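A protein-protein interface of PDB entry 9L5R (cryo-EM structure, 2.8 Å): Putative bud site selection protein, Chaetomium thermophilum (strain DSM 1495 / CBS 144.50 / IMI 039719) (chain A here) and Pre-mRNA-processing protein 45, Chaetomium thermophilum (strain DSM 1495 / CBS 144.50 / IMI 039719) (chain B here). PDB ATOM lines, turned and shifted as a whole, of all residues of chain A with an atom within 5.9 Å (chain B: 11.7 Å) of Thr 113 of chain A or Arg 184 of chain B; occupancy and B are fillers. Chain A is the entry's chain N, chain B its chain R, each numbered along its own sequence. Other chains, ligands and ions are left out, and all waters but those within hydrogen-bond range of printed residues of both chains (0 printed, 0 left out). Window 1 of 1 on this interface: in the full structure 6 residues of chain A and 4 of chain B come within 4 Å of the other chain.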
ATOM      1  N   GLN A 109     -21.481  28.551 -20.122  1.00  0.00           N
ATOM      2  CA  GLN A 109     -22.260  28.021 -19.001  1.00  0.00           C
ATOM      3  C   GLN A 109     -21.442  27.006 -18.203  1.00  0.00           C
ATOM      4  O   GLN A 109     -21.264  25.864 -18.631  1.00  0.00           O
ATOM      5  CB  GLN A 109     -23.549  27.399 -19.519  1.00  0.00           C
ATOM      6  CG  GLN A 109     -24.504  26.874 -18.462  1.00  0.00           C
ATOM      7  CD  GLN A 109     -24.834  27.868 -17.373  1.00  0.00           C
ATOM      8  OE1 GLN A 109     -24.805  27.535 -16.201  1.00  0.00           O
ATOM      9  NE2 GLN A 109     -25.165  29.084 -17.754  1.00  0.00           N
ATOM     10  N   THR A 110     -20.958  27.414 -17.029  1.00  0.00           N
ATOM     11  CA  THR A 110     -20.088  26.584 -16.206  1.00  0.00           C
ATOM     12  C   THR A 110     -20.836  25.658 -15.269  1.00  0.00           C
ATOM     13  O   THR A 110     -20.227  24.733 -14.733  1.00  0.00           O
ATOM     14  CB  THR A 110     -19.154  27.445 -15.355  1.00  0.00           C
ATOM     15  OG1 THR A 110     -19.918  28.416 -14.640  1.00  0.00           O
ATOM     16  CG2 THR A 110     -18.172  28.158 -16.211  1.00  0.00           C
ATOM     17  N   LYS A 111     -22.129  25.864 -15.050  1.00  0.00           N
ATOM     18  CA  LYS A 111     -22.828  24.919 -14.199  1.00  0.00           C
ATOM     19  C   LYS A 111     -23.105  23.605 -14.913  1.00  0.00           C
ATOM     20  O   LYS A 111     -23.477  22.633 -14.258  1.00  0.00           O
ATOM     21  CB  LYS A 111     -24.144  25.510 -13.681  1.00  0.00           C
ATOM     22  CG  LYS A 111     -24.003  26.758 -12.819  1.00  0.00           C
ATOM     23  CD  LYS A 111     -25.343  27.200 -12.206  1.00  0.00           C
ATOM     24  CE  LYS A 111     -26.396  27.763 -13.185  1.00  0.00           C
ATOM     25  NZ  LYS A 111     -26.112  29.066 -13.837  1.00  0.00           N
ATOM     26  N   GLU A 112     -22.903  23.548 -16.224  1.00  0.00           N
ATOM     27  CA  GLU A 112     -23.300  22.411 -17.035  1.00  0.00           C
ATOM     28  C   GLU A 112     -22.129  21.590 -17.548  1.00  0.00           C
ATOM     29  O   GLU A 112     -22.313  20.762 -18.437  1.00  0.00           O
ATOM     30  CB  GLU A 112     -24.143  22.887 -18.210  1.00  0.00           C
ATOM     31  CG  GLU A 112     -25.496  23.384 -17.805  1.00  0.00           C
ATOM     32  CD  GLU A 112     -26.342  23.774 -18.981  1.00  0.00           C
ATOM     33  OE1 GLU A 112     -25.883  23.629 -20.132  1.00  0.00           O
ATOM     34  OE2 GLU A 112     -27.471  24.229 -18.751  1.00  0.00           O
ATOM     35  N   THR A 113     -20.936  21.796 -17.021  1.00  0.00           N
ATOM     36  CA  THR A 113     -19.791  20.980 -17.370  1.00  0.00           C
ATOM     37  C   THR A 113     -19.408  20.101 -16.187  1.00  0.00           C
ATOM     38  O   THR A 113     -19.849  20.322 -15.057  1.00  0.00           O
ATOM     39  CB  THR A 113     -18.617  21.855 -17.809  1.00  0.00           C
ATOM     40  OG1 THR A 113     -18.439  22.908 -16.866  1.00  0.00           O
ATOM     41  CG2 THR A 113     -18.893  22.468 -19.164  1.00  0.00           C
ATOM     42  N   ASN A 114     -18.580  19.092 -16.468  1.00  0.00           N
ATOM     43  CA  ASN A 114     -18.263  18.062 -15.479  1.00  0.00           C
ATOM     44  C   ASN A 114     -17.514  18.629 -14.287  1.00  0.00           C
ATOM     45  O   ASN A 114     -17.757  18.224 -13.147  1.00  0.00           O
ATOM     46  CB  ASN A 114     -17.429  16.956 -16.118  1.00  0.00           C
ATOM     47  CG  ASN A 114     -18.254  15.977 -16.888  1.00  0.00           C
ATOM     48  OD1 ASN A 114     -19.354  15.627 -16.482  1.00  0.00           O
ATOM     49  ND2 ASN A 114     -17.725  15.512 -18.001  1.00  0.00           N
ATOM     50  N   PHE A 115     -16.590  19.551 -14.524  1.00  0.00           N
ATOM     51  CA  PHE A 115     -15.733  20.074 -13.472  1.00  0.00           C
ATOM     52  C   PHE A 115     -15.913  21.571 -13.308  1.00  0.00           C
ATOM     53  O   PHE A 115     -15.029  22.251 -12.789  1.00  0.00           O
ATOM     54  CB  PHE A 115     -14.280  19.714 -13.755  1.00  0.00           C
ATOM     55  CG  PHE A 115     -14.067  18.252 -13.869  1.00  0.00           C
ATOM     56  CD1 PHE A 115     -14.072  17.453 -12.745  1.00  0.00           C
ATOM     57  CD2 PHE A 115     -13.945  17.658 -15.107  1.00  0.00           C
ATOM     58  CE1 PHE A 115     -13.918  16.111 -12.858  1.00  0.00           C
ATOM     59  CE2 PHE A 115     -13.790  16.313 -15.214  1.00  0.00           C
ATOM     60  CZ  PHE A 115     -13.784  15.541 -14.093  1.00  0.00           C
ATOM     61  N   ASN A 116     -17.096  22.052 -13.684  1.00  0.00           N
ATOM     62  CA  ASN A 116     -17.468  23.479 -13.549  1.00  0.00           C
ATOM     63  C   ASN A 116     -16.446  24.300 -14.316  1.00  0.00           C
ATOM     64  O   ASN A 116     -15.961  25.283 -13.797  1.00  0.00           O
ATOM     65  CB  ASN A 116     -17.763  23.815 -12.095  1.00  0.00           C
ATOM     66  CG  ASN A 116     -18.929  23.038 -11.537  1.00  0.00           C
ATOM     67  OD1 ASN A 116     -20.048  23.155 -12.022  1.00  0.00           O
ATOM     68  ND2 ASN A 116     -18.673  22.244 -10.513  1.00  0.00           N
ATOM     69  N   SER A 117     -16.188  23.895 -15.543  1.00  0.00           N
ATOM     70  CA  SER A 117     -15.237  24.624 -16.399  1.00  0.00           C
ATOM     71  C   SER A 117     -15.975  25.267 -17.557  1.00  0.00           C
ATOM     72  O   SER A 117     -17.120  24.944 -17.760  1.00  0.00           O
ATOM     73  CB  SER A 117     -14.276  23.650 -16.938  1.00  0.00           C
ATOM     74  OG  SER A 117     -13.517  23.048 -15.904  1.00  0.00           O
ATOM     75  N   THR A 118     -15.352  26.184 -18.278  1.00  0.00           N
ATOM     76  CA  THR A 118     -15.965  26.692 -19.520  1.00  0.00           C
ATOM     77  C   THR A 118     -15.522  25.714 -20.590  1.00  0.00           C
ATOM     78  O   THR A 118     -14.882  24.722 -20.247  1.00  0.00           O
ATOM     79  CB  THR A 118     -15.494  28.104 -19.836  1.00  0.00           C
ATOM     80  OG1 THR A 118     -14.140  28.015 -20.268  1.00  0.00           O
ATOM     81  CG2 THR A 118     -15.604  29.037 -18.654  1.00  0.00           C
ATOM     82  N   CYS A 119     -15.808  25.961 -21.853  1.00  0.00           N
ATOM     83  CA  CYS A 119     -15.285  24.946 -22.790  1.00  0.00           C
ATOM     84  C   CYS A 119     -13.863  25.288 -23.198  1.00  0.00           C
ATOM     85  O   CYS A 119     -13.397  26.379 -22.877  1.00  0.00           O
ATOM     86  CB  CYS A 119     -16.130  24.761 -24.024  1.00  0.00           C
ATOM     87  SG  CYS A 119     -16.545  26.362 -24.689  1.00  0.00           S
ATOM     88  N   LYS B 176     -36.645  10.048  -5.724  1.00  0.00           N
ATOM     89  CA  LYS B 176     -36.823  11.477  -5.476  1.00  0.00           C
ATOM     90  C   LYS B 176     -37.116  12.209  -6.793  1.00  0.00           C
ATOM     91  O   LYS B 176     -36.464  13.167  -7.189  1.00  0.00           O
ATOM     92  CB  LYS B 176     -35.581  11.979  -4.724  1.00  0.00           C
ATOM     93  CG  LYS B 176     -35.450  13.431  -4.181  1.00  0.00           C
ATOM     94  CD  LYS B 176     -34.662  14.382  -5.064  1.00  0.00           C
ATOM     95  CE  LYS B 176     -33.193  14.020  -5.087  1.00  0.00           C
ATOM     96  NZ  LYS B 176     -32.417  14.934  -5.962  1.00  0.00           N
ATOM     97  N   GLN B 179     -33.472  12.344 -10.210  1.00  0.00           N
ATOM     98  CA  GLN B 179     -32.330  11.868  -9.436  1.00  0.00           C
ATOM     99  C   GLN B 179     -31.072  12.670  -9.754  1.00  0.00           C
ATOM    100  O   GLN B 179     -30.002  12.109  -9.985  1.00  0.00           O
ATOM    101  CB  GLN B 179     -32.108  10.385  -9.710  1.00  0.00           C
ATOM    102  CG  GLN B 179     -33.299   9.465  -9.392  1.00  0.00           C
ATOM    103  CD  GLN B 179     -33.690   9.438  -7.934  1.00  0.00           C
ATOM    104  OE1 GLN B 179     -34.732   9.959  -7.557  1.00  0.00           O
ATOM    105  NE2 GLN B 179     -32.863   8.820  -7.111  1.00  0.00           N
ATOM    106  N   VAL B 180     -31.175  13.995  -9.755  1.00  0.00           N
ATOM    107  CA  VAL B 180     -29.995  14.844  -9.819  1.00  0.00           C
ATOM    108  C   VAL B 180     -29.920  15.623  -8.521  1.00  0.00           C
ATOM    109  O   VAL B 180     -30.928  15.843  -7.840  1.00  0.00           O
ATOM    110  CB  VAL B 180     -29.960  15.802 -11.031  1.00  0.00           C
ATOM    111  CG1 VAL B 180     -30.241  15.045 -12.330  1.00  0.00           C
ATOM    112  CG2 VAL B 180     -30.892  16.993 -10.842  1.00  0.00           C
ATOM    113  N   ASN B 181     -28.703  16.006  -8.161  1.00  0.00           N
ATOM    114  CA  ASN B 181     -28.452  16.834  -6.992  1.00  0.00           C
ATOM    115  C   ASN B 181     -27.914  18.177  -7.454  1.00  0.00           C
ATOM    116  O   ASN B 181     -27.093  18.236  -8.375  1.00  0.00           O
ATOM    117  CB  ASN B 181     -27.469  16.150  -6.036  1.00  0.00           C
ATOM    118  CG  ASN B 181     -28.086  14.951  -5.318  1.00  0.00           C
ATOM    119  OD1 ASN B 181     -29.297  14.893  -5.110  1.00  0.00           O
ATOM    120  ND2 ASN B 181     -27.249  13.986  -4.946  1.00  0.00           N
ATOM    121  N   THR B 182     -28.407  19.254  -6.844  1.00  0.00           N
ATOM    122  CA  THR B 182     -27.827  20.571  -7.091  1.00  0.00           C
ATOM    123  C   THR B 182     -26.494  20.721  -6.367  1.00  0.00           C
ATOM    124  O   THR B 182     -25.527  21.256  -6.925  1.00  0.00           O
ATOM    125  CB  THR B 182     -28.809  21.661  -6.660  1.00  0.00           C
ATOM    126  OG1 THR B 182     -30.009  21.549  -7.432  1.00  0.00           O
ATOM    127  CG2 THR B 182     -28.215  23.044  -6.863  1.00  0.00           C
ATOM    128  N   LYS B 183     -26.417  20.218  -5.136  1.00  0.00           N
ATOM    129  CA  LYS B 183     -25.202  20.281  -4.338  1.00  0.00           C
ATOM    130  C   LYS B 183     -24.194  19.253  -4.839  1.00  0.00           C
ATOM    131  O   LYS B 183     -23.997  18.212  -4.208  1.00  0.00           O
ATOM    132  CB  LYS B 183     -25.538  20.036  -2.865  1.00  0.00           C
ATOM    133  CG  LYS B 183     -26.521  21.027  -2.196  1.00  0.00           C
ATOM    134  CD  LYS B 183     -25.976  22.444  -1.942  1.00  0.00           C
ATOM    135  CE  LYS B 183     -26.296  23.444  -3.057  1.00  0.00           C
ATOM    136  NZ  LYS B 183     -25.842  24.826  -2.719  1.00  0.00           N
ATOM    137  N   ARG B 184     -23.600  19.504  -6.003  1.00  0.00           N
ATOM    138  CA  ARG B 184     -22.632  18.586  -6.599  1.00  0.00           C
ATOM    139  C   ARG B 184     -21.203  19.103  -6.408  1.00  0.00           C
ATOM    140  O   ARG B 184     -20.471  19.364  -7.363  1.00  0.00           O
ATOM    141  CB  ARG B 184     -22.963  18.380  -8.071  1.00  0.00           C
ATOM    142  CG  ARG B 184     -22.465  17.092  -8.667  1.00  0.00           C
ATOM    143  CD  ARG B 184     -22.553  17.134 -10.185  1.00  0.00           C
ATOM    144  NE  ARG B 184     -21.649  18.132 -10.738  1.00  0.00           N
ATOM    145  CZ  ARG B 184     -20.830  17.928 -11.759  1.00  0.00           C
ATOM    146  NH1 ARG B 184     -20.750  16.754 -12.359  1.00  0.00           N
ATOM    147  NH2 ARG B 184     -20.062  18.926 -12.179  1.00  0.00           N
ATOM    148  N   GLU B 185     -20.794  19.222  -5.151  1.00  0.00           N
ATOM    149  CA  GLU B 185     -19.440  19.661  -4.848  1.00  0.00           C
ATOM    150  C   GLU B 185     -18.447  18.518  -5.031  1.00  0.00           C
ATOM    151  O   GLU B 185     -18.814  17.352  -5.192  1.00  0.00           O
ATOM    152  CB  GLU B 185     -19.345  20.215  -3.425  1.00  0.00           C
ATOM    153  CG  GLU B 185     -19.505  19.171  -2.326  1.00  0.00           C
ATOM    154  CD  GLU B 185     -20.957  18.891  -1.968  1.00  0.00           C
ATOM    155  OE1 GLU B 185     -21.852  19.265  -2.743  1.00  0.00           O
ATOM    156  OE2 GLU B 185     -21.208  18.294  -0.903  1.00  0.00           O
ATOM    157  N   ALA B 186     -17.169  18.872  -5.006  1.00  0.00           N
ATOM    158  CA  ALA B 186     -16.084  17.947  -5.273  1.00  0.00           C
ATOM    159  C   ALA B 186     -15.431  17.489  -3.979  1.00  0.00           C
ATOM    160  O   ALA B 186     -15.318  18.245  -3.013  1.00  0.00           O
ATOM    161  CB  ALA B 186     -15.032  18.593  -6.167  1.00  0.00           C
ATOM    162  N   THR B 187     -15.006  16.233  -3.972  1.00  0.00           N
ATOM    163  CA  THR B 187     -14.163  15.687  -2.924  1.00  0.00           C
ATOM    164  C   THR B 187     -12.719  15.748  -3.401  1.00  0.00           C
ATOM    165  O   THR B 187     -12.446  15.589  -4.592  1.00  0.00           O
ATOM    166  CB  THR B 187     -14.576  14.247  -2.612  1.00  0.00           C
ATOM    167  OG1 THR B 187     -15.937  14.232  -2.177  1.00  0.00           O
ATOM    168  CG2 THR B 187     -13.720  13.629  -1.528  1.00  0.00           C
ATOM    169  N   PHE B 188     -11.798  16.024  -2.486  1.00  0.00           N
ATOM    170  CA  PHE B 188     -10.379  15.959  -2.784  1.00  0.00           C
ATOM    171  C   PHE B 188      -9.749  14.818  -1.999  1.00  0.00           C
ATOM    172  O   PHE B 188     -10.098  14.583  -0.841  1.00  0.00           O
ATOM    173  CB  PHE B 188      -9.697  17.285  -2.469  1.00  0.00           C
ATOM    174  CG  PHE B 188     -10.046  18.381  -3.430  1.00  0.00           C
ATOM    175  CD1 PHE B 188      -9.487  18.415  -4.690  1.00  0.00           C
ATOM    176  CD2 PHE B 188     -10.948  19.367  -3.080  1.00  0.00           C
ATOM    177  CE1 PHE B 188      -9.810  19.410  -5.576  1.00  0.00           C
ATOM    178  CE2 PHE B 188     -11.268  20.367  -3.965  1.00  0.00           C
ATOM    179  CZ  PHE B 188     -10.695  20.387  -5.213  1.00  0.00           C
ATOM    180  N   LYS B 209      -9.377  15.110  -7.671  1.00  0.00           N
ATOM    181  CA  LYS B 209     -10.645  15.826  -7.590  1.00  0.00           C
ATOM    182  C   LYS B 209     -11.743  14.915  -8.120  1.00  0.00           C
ATOM    183  O   LYS B 209     -11.821  14.670  -9.324  1.00  0.00           O
ATOM    184  CB  LYS B 209     -10.594  17.122  -8.392  1.00  0.00           C
ATOM    185  CG  LYS B 209     -11.835  17.963  -8.254  1.00  0.00           C
ATOM    186  CD  LYS B 209     -11.630  19.329  -8.826  1.00  0.00           C
ATOM    187  CE  LYS B 209     -12.908  19.874  -9.412  1.00  0.00           C
ATOM    188  NZ  LYS B 209     -12.625  21.046 -10.266  1.00  0.00           N
ATOM    189  N   ILE B 210     -12.603  14.435  -7.234  1.00  0.00           N
ATOM    190  CA  ILE B 210     -13.655  13.497  -7.591  1.00  0.00           C
ATOM    191  C   ILE B 210     -14.985  14.227  -7.525  1.00  0.00           C
ATOM    192  O   ILE B 210     -15.356  14.759  -6.473  1.00  0.00           O
ATOM    193  CB  ILE B 210     -13.663  12.270  -6.668  1.00  0.00           C
ATOM    194  CG1 ILE B 210     -12.269  11.648  -6.593  1.00  0.00           C
ATOM    195  CG2 ILE B 210     -14.674  11.259  -7.149  1.00  0.00           C
ATOM    196  CD1 ILE B 210     -12.193  10.431  -5.723  1.00  0.00           C
ATOM    197  N   VAL B 211     -15.704  14.248  -8.643  1.00  0.00           N
ATOM    198  CA  VAL B 211     -17.062  14.772  -8.691  1.00  0.00           C
ATOM    199  C   VAL B 211     -18.000  13.657  -9.130  1.00  0.00           C
ATOM    200  O   VAL B 211     -17.619  12.751  -9.873  1.00  0.00           O
ATOM    201  CB  VAL B 211     -17.180  16.008  -9.617  1.00  0.00           C
ATOM    202  CG1 VAL B 211     -16.115  17.005  -9.287  1.00  0.00           C
ATOM    203  CG2 VAL B 211     -17.054  15.627 -11.069  1.00  0.00           C
ATOM    204  N   GLU B 212     -19.219  13.691  -8.604  1.00  0.00           N
ATOM    205  CA  GLU B 212     -20.269  12.796  -9.062  1.00  0.00           C
ATOM    206  C   GLU B 212     -20.757  13.243 -10.434  1.00  0.00           C
ATOM    207  O   GLU B 212     -20.968  14.428 -10.674  1.00  0.00           O
ATOM    208  CB  GLU B 212     -21.414  12.782  -8.053  1.00  0.00           C
ATOM    209  CG  GLU B 212     -22.492  11.755  -8.307  1.00  0.00           C
ATOM    210  CD  GLU B 212     -23.748  12.013  -7.491  1.00  0.00           C
ATOM    211  OE1 GLU B 212     -23.651  12.070  -6.249  1.00  0.00           O
ATOM    212  OE2 GLU B 212     -24.837  12.172  -8.082  1.00  0.00           O
ATOM    213  N   ARG B 213     -20.917  12.293 -11.345  1.00  0.00           N
ATOM    214  CA  ARG B 213     -21.205  12.616 -12.736  1.00  0.00           C
ATOM    215  C   ARG B 213     -22.638  13.106 -12.911  1.00  0.00           C
ATOM    216  O   ARG B 213     -23.563  12.615 -12.263  1.00  0.00           O
ATOM    217  CB  ARG B 213     -20.949  11.386 -13.600  1.00  0.00           C
ATOM    218  CG  ARG B 213     -21.370  11.477 -15.042  1.00  0.00           C
ATOM    219  CD  ARG B 213     -21.327  10.105 -15.662  1.00  0.00           C
ATOM    220  NE  ARG B 213     -21.443  10.110 -17.114  1.00  0.00           N
ATOM    221  CZ  ARG B 213     -20.445  10.361 -17.950  1.00  0.00           C
ATOM    222  NH1 ARG B 213     -19.241  10.687 -17.513  1.00  0.00           N
ATOM    223  NH2 ARG B 213     -20.659  10.276 -19.260  1.00  0.00           N
ATOM    224  N   GLN B 214     -22.817  14.105 -13.778  1.00  0.00           N
ATOM    225  CA  GLN B 214     -24.148  14.559 -14.182  1.00  0.00           C
ATOM    226  C   GLN B 214     -24.822  13.477 -15.013  1.00  0.00           C
ATOM    227  O   GLN B 214     -24.460  13.270 -16.172  1.00  0.00           O
ATOM    228  CB  GLN B 214     -24.047  15.840 -15.000  1.00  0.00           C
ATOM    229  CG  GLN B 214     -23.432  17.033 -14.310  1.00  0.00           C
ATOM    230  CD  GLN B 214     -22.836  18.041 -15.297  1.00  0.00           C
ATOM    231  OE1 GLN B 214     -22.523  17.707 -16.441  1.00  0.00           O
ATOM    232  NE2 GLN B 214     -22.680  19.279 -14.847  1.00  0.00           N
ATOM    233  N   ARG B 215     -25.797  12.790 -14.449  1.00  0.00           N
ATOM    234  CA  ARG B 215     -26.541  11.814 -15.224  1.00  0.00           C
ATOM    235  C   ARG B 215     -27.845  12.418 -15.730  1.00  0.00           C
ATOM    236  O   ARG B 215     -28.425  13.304 -15.103  1.00  0.00           O
ATOM    237  CB  ARG B 215     -26.798  10.538 -14.417  1.00  0.00           C
ATOM    238  CG  ARG B 215     -27.771  10.645 -13.266  1.00  0.00           C
ATOM    239  CD  ARG B 215     -28.014   9.261 -12.661  1.00  0.00           C
ATOM    240  NE  ARG B 215     -27.055   8.925 -11.614  1.00  0.00           N
ATOM    241  CZ  ARG B 215     -26.373   7.788 -11.549  1.00  0.00           C
ATOM    242  NH1 ARG B 215     -26.521   6.839 -12.455  1.00  0.00           N
ATOM    243  NH2 ARG B 215     -25.522   7.600 -10.545  1.00  0.00           N
ATOM    244  N   ASP B 216     -28.256  11.960 -16.902  1.00  0.00           N
ATOM    245  CA  ASP B 216     -29.484  12.375 -17.564  1.00  0.00           C
ATOM    246  C   ASP B 216     -30.694  11.999 -16.717  1.00  0.00           C
ATOM    247  O   ASP B 216     -30.879  10.815 -16.415  1.00  0.00           O
ATOM    248  CB  ASP B 216     -29.524  11.696 -18.934  1.00  0.00           C
ATOM    249  CG  ASP B 216     -30.661  12.158 -19.816  1.00  0.00           C
ATOM    250  OD1 ASP B 216     -31.326  13.148 -19.515  1.00  0.00           O
ATOM    251  OD2 ASP B 216     -30.900  11.510 -20.841  1.00  0.00           O
ATOM    252  N   PRO B 217     -31.541  12.957 -16.325  1.00  0.00           N
ATOM    253  CA  PRO B 217     -32.640  12.644 -15.404  1.00  0.00           C
ATOM    254  C   PRO B 217     -33.739  11.790 -16.015  1.00  0.00           C
ATOM    255  O   PRO B 217     -34.570  11.269 -15.271  1.00  0.00           O
ATOM    256  CB  PRO B 217     -33.179  14.025 -15.024  1.00  0.00           C
ATOM    257  CG  PRO B 217     -32.186  14.985 -15.502  1.00  0.00           C
ATOM    258  CD  PRO B 217     -31.496  14.392 -16.638  1.00  0.00           C
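The backbone carbonyl oxygen of Asn 114 of chain A lies within hydrogen-bond range of the guanidinium group of Arg 184 of chain B, at 2.6 Å. O of Thr 113 of chain A sits at hydrogen-bond distance from NE2 of Gln 214 of chain B. The side-chain amide nitrogen of Gln 214 of chain B lies within hydrogen-bond range of the backbone carbonyl oxygen of Lys 111 of chain A, 3.5 Å away. The backbone carbonyl oxygen (O) of Thr 113 of chain A sits at hydrogen-bond distance from the guanidinium group (NH2) of Arg 184 of chain B (3.2 Å).
OE1 of Gln 109 of chain A is in hydrogen-bond range of NZ of Lys 111 of chain A (3.1 Å). O of Thr 110 of chain A lies within hydrogen-bond range of OG1 of Thr 113 of chain A (3.3 Å). O of Ser 117 of chain A lies within hydrogen-bond range of OG1 of Thr 113 of chain A (2.6 Å). The backbone carbonyl oxygen (O) of Glu 212 of chain B is in hydrogen-bond range of the guanidinium group (NH1) of Arg 184 of chain B, at 2.9 Å. The backbone carbonyl oxygen (O) of Thr 110 of chain A lies close to the side-chain amide oxygen (OD1) of Asn 116 of chain A, 3.1 Å away.
Among the printed residues, merely in contact across the chains: Asn 114 of chain A with Val 211 of chain B, Glu 112 of chain A with Gln 214 of chain B, Phe 115 of chain A with Val 211 of chain B, Phe 115 of chain A with Lys 209 of chain B, Asn 114 of chain A with Gln 214 of chain B and Asn 116 of chain A with Arg 184 of chain B.
Of chain B, only Arg 184 (3.2 Å) and Gln 214 (3.0 Å) come within 4 Å of Thr 113 of chain A. Arg 184 of chain B touches just these residues of chain A: Thr 113 (3.2 Å), Asn 114 (2.6 Å) and Asn 116 (3.96 Å). No residue of chain B comes within 4 Å of Thr 110 of chain A. Asn 114 of chain A touches just these residues of chain B: Arg 184, Val 211 and Gln 214. Of the printed residues of chain B, Phe 115 of chain A touches Lys 209 and Val 211. Asn 116 of chain A touches just one residue of chain B: Arg 184. No residue of chain B comes within 4 Å of Ser 117 of chain A. Of the printed residues of chain A, Gln 214 of chain B touches Lys 111, Glu 112, Thr 113 and Asn 114. Printed residues of chain A within 4 Å of Lys 209 of chain B: Phe 115 (3.7 Å). Of the printed residues of chain B, Lys 111 of chain A touches Gln 214. Arg 213 of chain B touches none of the printed residues of chain A.
Of the 11 printed residues of chain A, 6 touch a printed residue of chain B. Hydrophobic or aromatic side chains of chain A that line the printed part of chain B: Phe 115. Hydrophobic or aromatic side chains of chain B within 4 Å of the printed part of chain A: Val 211.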
